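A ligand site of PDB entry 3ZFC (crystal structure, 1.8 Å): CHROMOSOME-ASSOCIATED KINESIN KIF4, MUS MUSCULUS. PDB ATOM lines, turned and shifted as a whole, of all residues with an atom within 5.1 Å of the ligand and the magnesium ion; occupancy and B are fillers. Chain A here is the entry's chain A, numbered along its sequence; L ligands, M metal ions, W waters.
The magnesium ion is bound by O3 of the ligand (2.0 Å), water W4 (2.1 Å), O5 of the ligand (2.1 Å), OG1 of Thr 95 (2.1 Å), water W7 (2.1 Å) and OG of Ser 211 (2.1 Å).
Within 4 Å of the magnesium ion: Thr 95 and Ser 211. Along chain A the residues within 4 Å of the magnesium ion span positions 95 to 211. The nearest printed residue that does not touch the magnesium ion is Asp 241 (4.3 Å).
N of Gly 91 lies close to N1 of the ligand, at 2.8 Å. Merely in contact with the ligand: Arg 15, Arg 17, Pro 18, Val 20 and Gln 89. Hydrophobic or aromatic side chains within 4 Å of the ligand: Pro 18, Val 20 and Tyr 96.
Water W4 lies within hydrogen-bond range of O7 of the ligand (2.7 Å) and O of Gln 209 (2.9 Å). Water W7 lies within hydrogen-bond range of the side-chain carboxylate of Asp 241 (2.7 Å) and the backbone carbonyl oxygen of Leu 242 (2.7 Å). Water W1 lies within hydrogen-bond range of O of Ser 211 (2.6 Å), O2 of the ligand (2.7 Å) and N of Gly 244 (2.9 Å). Water W2 lies within hydrogen-bond range of the side-chain amide oxygen (OD1) of Asn 207 (2.7 Å) and an oxygen (O11) of the ligand (2.8 Å). Water W5 lies within hydrogen-bond range of N3 of the ligand (2.9 Å), OG of Ser 97 (3.1 Å) and NH1 of Arg 15 (3.4 Å).
N of Thr 95 sits at hydrogen-bond distance from OD1 of Asp 241, at 3.4 Å. O of Gly 91 sits at hydrogen-bond distance from NE of Arg 17, at 2.7 Å. The side-chain amino group of Lys 94 is in hydrogen-bond range of the backbone carbonyl oxygen of Gln 89 (3.0 Å). The side-chain amino group (NZ) of Lys 94 is in hydrogen-bond range of the backbone carbonyl oxygen (O) of Gly 88 (2.9 Å). O of Gly 93 is in hydrogen-bond range of OG of Ser 97 (2.7 Å). N of Gln 209 sits at hydrogen-bond distance from OD1 of Asn 207 (2.9 Å). The side-chain hydroxyl of Ser 92 is in hydrogen-bond range of the backbone carbonyl oxygen of Gln 89 (2.7 Å). The guanidinium group (NH1) of Arg 15 lies within hydrogen-bond range of the side-chain hydroxyl (OG) of Ser 97 (3.0 Å).
N of Thr 95 is in hydrogen-bond range of O6 of the ligand. The backbone NH (N) of Ser 211 sits close to an oxygen (O3) of the ligand (2.8 Å). O1 of the ligand sits at hydrogen-bond distance from OG of Ser 210, 2.7 Å away. OG1 of Thr 90 lies within hydrogen-bond range of O1 of the ligand (2.7 Å). N of Tyr 96 sits at hydrogen-bond distance from O6 of the ligand, at 2.8 Å. The backbone NH of Lys 94 sits at hydrogen-bond distance from an oxygen (O4) of the ligand, 2.9 Å away. O4 of the ligand lies within salt-bridge range of NZ of Lys 94, 2.8 Å away. An oxygen (O4) of the ligand lies within hydrogen-bond range of the backbone NH (N) of Gly 93, 2.9 Å away. O7 of the ligand is in hydrogen-bond range of ND2 of Asn 207, 3.0 Å away. An oxygen (O2) of the ligand is in hydrogen-bond range of the backbone NH of Gly 244 (3.2 Å). O4 of the ligand sits at hydrogen-bond distance from N of Ser 92, 3.3 Å away.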
ATOM      1  N   ARG A  15       1.159  14.958  14.322  1.00  0.00           N
ATOM      2  CA  ARG A  15       1.912  15.907  15.100  1.00  0.00           C
ATOM      3  C   ARG A  15       1.046  16.604  16.114  1.00  0.00           C
ATOM      4  O   ARG A  15       0.146  17.370  15.764  1.00  0.00           O
ATOM      5  CB  ARG A  15       2.661  16.918  14.254  1.00  0.00           C
ATOM      6  CG  ARG A  15       3.690  17.614  15.130  1.00  0.00           C
ATOM      7  CD  ARG A  15       4.128  18.948  14.637  1.00  0.00           C
ATOM      8  NE  ARG A  15       5.329  19.374  15.358  1.00  0.00           N
ATOM      9  CZ  ARG A  15       6.126  20.338  14.952  1.00  0.00           C
ATOM     10  NH1 ARG A  15       5.836  21.049  13.846  1.00  0.00           N
ATOM     11  NH2 ARG A  15       7.230  20.592  15.646  1.00  0.00           N
ATOM     12  N   ARG A  17       0.988  19.365  18.943  1.00  0.00           N
ATOM     13  CA  ARG A  17       1.686  20.534  19.417  1.00  0.00           C
ATOM     14  C   ARG A  17       1.531  20.613  20.943  1.00  0.00           C
ATOM     15  O   ARG A  17       0.692  19.942  21.505  1.00  0.00           O
ATOM     16  CB  ARG A  17       1.137  21.803  18.777  1.00  0.00           C
ATOM     17  CG  ARG A  17      -0.332  22.128  19.010  1.00  0.00           C
ATOM     18  CD  ARG A  17      -0.587  23.618  18.973  1.00  0.00           C
ATOM     19  NE  ARG A  17      -2.006  23.997  18.974  1.00  0.00           N
ATOM     20  CZ  ARG A  17      -2.827  23.943  20.022  1.00  0.00           C
ATOM     21  NH1 ARG A  17      -2.412  23.560  21.235  1.00  0.00           N
ATOM     22  NH2 ARG A  17      -4.096  24.287  19.871  1.00  0.00           N
ATOM     23  N   PRO A  18       2.328  21.464  21.600  1.00  0.00           N
ATOM     24  CA  PRO A  18       2.051  21.729  23.009  1.00  0.00           C
ATOM     25  C   PRO A  18       0.772  22.466  23.247  1.00  0.00           C
ATOM     26  O   PRO A  18       0.240  23.147  22.328  1.00  0.00           O
ATOM     27  CB  PRO A  18       3.191  22.629  23.453  1.00  0.00           C
ATOM     28  CG  PRO A  18       4.129  22.706  22.321  1.00  0.00           C
ATOM     29  CD  PRO A  18       3.425  22.306  21.092  1.00  0.00           C
ATOM     30  N   VAL A  20      -1.361  25.519  24.163  1.00  0.00           N
ATOM     31  CA  VAL A  20      -1.152  26.930  23.859  1.00  0.00           C
ATOM     32  C   VAL A  20      -1.807  27.797  24.946  1.00  0.00           C
ATOM     33  O   VAL A  20      -2.517  27.280  25.809  1.00  0.00           O
ATOM     34  CB  VAL A  20      -1.714  27.320  22.467  1.00  0.00           C
ATOM     35  CG1 VAL A  20      -0.898  26.661  21.363  1.00  0.00           C
ATOM     36  CG2 VAL A  20      -3.191  26.981  22.327  1.00  0.00           C
ATOM     37  N   GLY A  88      -5.783  19.630   9.841  1.00  0.00           N
ATOM     38  CA  GLY A  88      -6.234  19.645  11.250  1.00  0.00           C
ATOM     39  C   GLY A  88      -7.042  20.895  11.588  1.00  0.00           C
ATOM     40  O   GLY A  88      -7.144  21.827  10.791  1.00  0.00           O
ATOM     41  N   GLN A  89      -7.569  20.914  12.825  1.00  0.00           N
ATOM     42  CA  GLN A  89      -8.408  21.986  13.349  1.00  0.00           C
ATOM     43  C   GLN A  89      -7.679  23.342  13.298  1.00  0.00           C
ATOM     44  O   GLN A  89      -6.455  23.408  13.398  1.00  0.00           O
ATOM     45  CB  GLN A  89      -8.706  21.617  14.785  1.00  0.00           C
ATOM     46  CG  GLN A  89      -9.369  22.643  15.604  1.00  0.00           C
ATOM     47  CD  GLN A  89      -9.373  22.324  17.073  1.00  0.00           C
ATOM     48  OE1 GLN A  89      -8.498  21.618  17.638  1.00  0.00           O
ATOM     49  NE2 GLN A  89     -10.372  22.852  17.712  1.00  0.00           N
ATOM     50  N   THR A  90      -8.429  24.432  13.163  1.00  0.00           N
ATOM     51  CA  THR A  90      -7.834  25.746  13.397  1.00  0.00           C
ATOM     52  C   THR A  90      -6.982  25.751  14.702  1.00  0.00           C
ATOM     53  O   THR A  90      -7.382  25.240  15.763  1.00  0.00           O
ATOM     54  CB  THR A  90      -8.896  26.877  13.428  1.00  0.00           C
ATOM     55  OG1 THR A  90      -8.252  28.159  13.599  1.00  0.00           O
ATOM     56  CG2 THR A  90      -9.904  26.700  14.587  1.00  0.00           C
ATOM     57  N   GLY A  91      -5.792  26.326  14.607  1.00  0.00           N
ATOM     58  CA  GLY A  91      -4.916  26.492  15.756  1.00  0.00           C
ATOM     59  C   GLY A  91      -4.077  25.263  16.066  1.00  0.00           C
ATOM     60  O   GLY A  91      -3.289  25.295  16.998  1.00  0.00           O
ATOM     61  N   SER A  92      -4.239  24.183  15.314  1.00  0.00           N
ATOM     62  CA  SER A  92      -3.547  22.944  15.630  1.00  0.00           C
ATOM     63  C   SER A  92      -2.045  22.918  15.294  1.00  0.00           C
ATOM     64  O   SER A  92      -1.329  22.069  15.851  1.00  0.00           O
ATOM     65  CB  SER A  92      -4.272  21.746  15.014  1.00  0.00           C
ATOM     66  OG  SER A  92      -4.293  21.820  13.592  1.00  0.00           O
ATOM     67  N   GLY A  93      -1.607  23.777  14.372  1.00  0.00           N
ATOM     68  CA  GLY A  93      -0.196  23.903  13.965  1.00  0.00           C
ATOM     69  C   GLY A  93       0.208  23.586  12.531  1.00  0.00           C
ATOM     70  O   GLY A  93       1.385  23.281  12.272  1.00  0.00           O
ATOM     71  N   LYS A  94      -0.745  23.688  11.591  1.00  0.00           N
ATOM     72  CA  LYS A  94      -0.483  23.411  10.178  1.00  0.00           C
ATOM     73  C   LYS A  94       0.525  24.436   9.632  1.00  0.00           C
ATOM     74  O   LYS A  94       1.546  24.072   9.063  1.00  0.00           O
ATOM     75  CB  LYS A  94      -1.764  23.507   9.366  1.00  0.00           C
ATOM     76  CG  LYS A  94      -2.866  22.548   9.834  1.00  0.00           C
ATOM     77  CD  LYS A  94      -4.134  22.695   9.008  1.00  0.00           C
ATOM     78  CE  LYS A  94      -4.878  23.992   9.272  1.00  0.00           C
ATOM     79  NZ  LYS A  94      -5.315  24.086  10.670  1.00  0.00           N
ATOM     80  N   THR A  95       0.202  25.705   9.798  1.00  0.00           N
ATOM     81  CA  THR A  95       1.047  26.801   9.250  1.00  0.00           C
ATOM     82  C   THR A  95       2.425  26.771   9.915  1.00  0.00           C
ATOM     83  O   THR A  95       3.456  26.870   9.230  1.00  0.00           O
ATOM     84  CB  THR A  95       0.325  28.133   9.429  1.00  0.00           C
ATOM     85  OG1 THR A  95      -0.871  28.105   8.627  1.00  0.00           O
ATOM     86  CG2 THR A  95       1.201  29.321   8.957  1.00  0.00           C
ATOM     87  N   TYR A  96       2.434  26.648  11.248  1.00  0.00           N
ATOM     88  CA  TYR A  96       3.669  26.460  11.990  1.00  0.00           C
ATOM     89  C   TYR A  96       4.509  25.305  11.440  1.00  0.00           C
ATOM     90  O   TYR A  96       5.708  25.476  11.171  1.00  0.00           O
ATOM     91  CB  TYR A  96       3.341  26.217  13.460  1.00  0.00           C
ATOM     92  CG  TYR A  96       4.570  26.008  14.282  1.00  0.00           C
ATOM     93  CD1 TYR A  96       5.275  27.104  14.772  1.00  0.00           C
ATOM     94  CD2 TYR A  96       5.045  24.745  14.554  1.00  0.00           C
ATOM     95  CE1 TYR A  96       6.424  26.934  15.506  1.00  0.00           C
ATOM     96  CE2 TYR A  96       6.207  24.574  15.301  1.00  0.00           C
ATOM     97  CZ  TYR A  96       6.868  25.671  15.791  1.00  0.00           C
ATOM     98  OH  TYR A  96       8.017  25.543  16.539  1.00  0.00           O
ATOM     99  N   SER A  97       3.876  24.151  11.251  1.00  0.00           N
ATOM    100  CA  SER A  97       4.583  22.971  10.801  1.00  0.00           C
ATOM    101  C   SER A  97       5.106  23.111   9.370  1.00  0.00           C
ATOM    102  O   SER A  97       6.173  22.604   9.038  1.00  0.00           O
ATOM    103  CB  SER A  97       3.676  21.728  10.860  1.00  0.00           C
ATOM    104  OG  SER A  97       3.331  21.369  12.193  1.00  0.00           O
ATOM    105  N   ARG A 199      -0.868  36.014   1.534  1.00  0.00           N
ATOM    106  CA  ARG A 199      -1.805  34.967   1.962  1.00  0.00           C
ATOM    107  C   ARG A 199      -2.797  35.587   2.939  1.00  0.00           C
ATOM    108  O   ARG A 199      -2.424  36.409   3.783  1.00  0.00           O
ATOM    109  CB  ARG A 199      -1.009  33.792   2.565  1.00  0.00           C
ATOM    110  CG  ARG A 199      -1.645  32.414   2.430  1.00  0.00           C
ATOM    111  CD  ARG A 199      -2.452  32.089   3.656  1.00  0.00           C
ATOM    112  NE  ARG A 199      -2.988  30.718   3.720  1.00  0.00           N
ATOM    113  CZ  ARG A 199      -2.342  29.664   4.214  1.00  0.00           C
ATOM    114  NH1 ARG A 199      -1.079  29.772   4.564  1.00  0.00           N
ATOM    115  NH2 ARG A 199      -2.945  28.493   4.299  1.00  0.00           N
ATOM    116  N   ASN A 207      -7.388  31.447  16.843  1.00  0.00           N
ATOM    117  CA  ASN A 207      -6.057  31.709  16.283  1.00  0.00           C
ATOM    118  C   ASN A 207      -5.969  33.148  15.788  1.00  0.00           C
ATOM    119  O   ASN A 207      -6.685  33.559  14.876  1.00  0.00           O
ATOM    120  CB  ASN A 207      -5.739  30.696  15.136  1.00  0.00           C
ATOM    121  CG  ASN A 207      -4.295  30.761  14.670  1.00  0.00           C
ATOM    122  OD1 ASN A 207      -3.510  31.672  15.051  1.00  0.00           O
ATOM    123  ND2 ASN A 207      -3.930  29.804  13.836  1.00  0.00           N
ATOM    124  N   GLN A 209      -3.722  34.448  14.176  1.00  0.00           N
ATOM    125  CA  GLN A 209      -3.115  34.420  12.844  1.00  0.00           C
ATOM    126  C   GLN A 209      -3.661  33.233  12.024  1.00  0.00           C
ATOM    127  O   GLN A 209      -2.903  32.474  11.361  1.00  0.00           O
ATOM    128  CB  GLN A 209      -1.601  34.253  12.984  1.00  0.00           C
ATOM    129  CG  GLN A 209      -0.922  35.343  13.798  1.00  0.00           C
ATOM    130  CD  GLN A 209      -0.734  36.668  13.100  1.00  0.00           C
ATOM    131  OE1 GLN A 209      -0.275  37.647  13.739  1.00  0.00           O
ATOM    132  NE2 GLN A 209      -1.008  36.725  11.823  1.00  0.00           N
ATOM    133  N   SER A 210      -4.969  33.118  12.023  1.00  0.00           N
ATOM    134  CA  SER A 210      -5.646  32.041  11.294  1.00  0.00           C
ATOM    135  C   SER A 210      -5.491  32.222   9.799  1.00  0.00           C
ATOM    136  O   SER A 210      -5.667  33.312   9.265  1.00  0.00           O
ATOM    137  CB  SER A 210      -7.117  32.039  11.614  1.00  0.00           C
ATOM    138  OG  SER A 210      -7.738  30.988  10.901  1.00  0.00           O
ATOM    139  N   SER A 211      -5.155  31.139   9.124  1.00  0.00           N
ATOM    140  CA  SER A 211      -5.143  31.116   7.662  1.00  0.00           C
ATOM    141  C   SER A 211      -6.566  31.071   7.145  1.00  0.00           C
ATOM    142  O   SER A 211      -7.323  30.156   7.450  1.00  0.00           O
ATOM    143  CB  SER A 211      -4.400  29.868   7.164  1.00  0.00           C
ATOM    144  OG  SER A 211      -3.145  29.682   7.788  1.00  0.00           O
ATOM    145  N   ASP A 241      -0.468  23.948   2.823  1.00  0.00           N
ATOM    146  CA  ASP A 241      -0.877  24.432   4.134  1.00  0.00           C
ATOM    147  C   ASP A 241      -2.408  24.687   4.058  1.00  0.00           C
ATOM    148  O   ASP A 241      -2.893  25.762   3.656  1.00  0.00           O
ATOM    149  CB  ASP A 241      -0.097  25.700   4.501  1.00  0.00           C
ATOM    150  CG  ASP A 241      -0.489  26.281   5.824  1.00  0.00           C
ATOM    151  OD1 ASP A 241      -1.052  25.527   6.652  1.00  0.00           O
ATOM    152  OD2 ASP A 241      -0.266  27.518   6.045  1.00  0.00           O
ATOM    153  N   LEU A 242      -3.184  23.664   4.392  1.00  0.00           N
ATOM    154  CA  LEU A 242      -4.649  23.789   4.311  1.00  0.00           C
ATOM    155  C   LEU A 242      -5.134  24.774   5.355  1.00  0.00           C
ATOM    156  O   LEU A 242      -4.518  24.938   6.401  1.00  0.00           O
ATOM    157  CB  LEU A 242      -5.350  22.434   4.586  1.00  0.00           C
ATOM    158  CG  LEU A 242      -5.122  21.268   3.601  1.00  0.00           C
ATOM    159  CD1 LEU A 242      -5.798  20.025   4.137  1.00  0.00           C
ATOM    160  CD2 LEU A 242      -5.662  21.627   2.232  1.00  0.00           C
ATOM    161  N   ALA A 243      -6.285  25.399   5.110  1.00  0.00           N
ATOM    162  CA  ALA A 243      -7.049  25.966   6.189  1.00  0.00           C
ATOM    163  C   ALA A 243      -7.645  24.840   7.063  1.00  0.00           C
ATOM    164  O   ALA A 243      -7.553  23.665   6.725  1.00  0.00           O
ATOM    165  CB  ALA A 243      -8.122  26.918   5.658  1.00  0.00           C
ATOM    166  N   GLY A 244      -8.151  25.191   8.227  1.00  0.00           N
ATOM    167  CA  GLY A 244      -8.561  24.232   9.220  1.00  0.00           C
ATOM    168  C   GLY A 244     -10.001  24.419   9.645  1.00  0.00           C
ATOM    169  O   GLY A 244     -10.551  25.519   9.558  1.00  0.00           O
HETATM  170  P1  LIG L   1      -5.501  27.864  11.085  1.00  0.00           P
HETATM  171  O1  LIG L   1      -6.374  28.873  11.771  1.00  0.00           O
HETATM  172  O2  LIG L   1      -6.374  26.698  10.488  1.00  0.00           O
HETATM  173  O3  LIG L   1      -4.712  28.471   9.970  1.00  0.00           O
HETATM  174  P2  LIG L   1      -3.082  26.438  12.085  1.00  0.00           P
HETATM  175  O4  LIG L   1      -3.232  24.947  12.304  1.00  0.00           O
HETATM  176  O5  LIG L   1      -2.327  26.916  10.838  1.00  0.00           O
HETATM  177  N1  LIG L   1      -4.564  27.187  12.265  1.00  0.00           N
HETATM  178  P3  LIG L   1      -0.876  27.718  13.420  1.00  0.00           P
HETATM  179  O6  LIG L   1       0.145  26.871  12.762  1.00  0.00           O
HETATM  180  O7  LIG L   1      -1.146  29.147  13.024  1.00  0.00           O
HETATM  181  O8  LIG L   1      -2.292  26.917  13.434  1.00  0.00           O
HETATM  182  O9  LIG L   1      -0.563  27.604  15.011  1.00  0.00           O
HETATM  183  C1  LIG L   1      -1.362  28.250  16.006  1.00  0.00           C
HETATM  184  C2  LIG L   1      -0.441  28.811  17.093  1.00  0.00           C
HETATM  185  O10 LIG L   1       0.151  27.707  17.776  1.00  0.00           O
HETATM  186  C3  LIG L   1       0.686  29.643  16.518  1.00  0.00           C
HETATM  187  O11 LIG L   1       0.886  30.821  17.349  1.00  0.00           O
HETATM  188  C4  LIG L   1       1.871  28.724  16.543  1.00  0.00           C
HETATM  189  O12 LIG L   1       3.123  29.445  16.618  1.00  0.00           O
HETATM  190  C5  LIG L   1       1.574  27.781  17.708  1.00  0.00           C
HETATM  191  N2  LIG L   1       2.103  26.432  17.481  1.00  0.00           N
HETATM  192  C6  LIG L   1       1.652  25.570  16.554  1.00  0.00           C
HETATM  193  N3  LIG L   1       2.347  24.442  16.570  1.00  0.00           N
HETATM  194  C7  LIG L   1       3.302  24.573  17.528  1.00  0.00           C
HETATM  195  C8  LIG L   1       4.397  23.734  18.053  1.00  0.00           C
HETATM  196  N4  LIG L   1       4.624  22.502  17.588  1.00  0.00           N
HETATM  197  N5  LIG L   1       5.185  24.244  19.043  1.00  0.00           N
HETATM  198  C9  LIG L   1       4.987  25.466  19.534  1.00  0.00           C
HETATM  199  N6  LIG L   1       3.985  26.279  19.102  1.00  0.00           N
HETATM  200  C10 LIG L   1       3.156  25.878  18.100  1.00  0.00           C
HETATM  201 MG    MG M   1      -2.838  28.269   9.369  1.00  0.00          MG
HETATM  202  O   HOH W   1      -8.066  28.021   8.808  1.00  0.00           O
HETATM  203  O   HOH W   2      -1.143  32.452  16.190  1.00  0.00           O
HETATM  204  O   HOH W   3       0.744  31.016  12.207  1.00  0.00           O
HETATM  205  O   HOH W   4      -2.168  29.771  10.604  1.00  0.00           O
HETATM  206  O   HOH W   5       2.883  21.903  15.241  1.00  0.00           O
HETATM  207  O   HOH W   6       2.946  28.112  21.420  1.00  0.00           O
HETATM  208  O   HOH W   7      -3.128  26.691   7.950  1.00  0.00           O
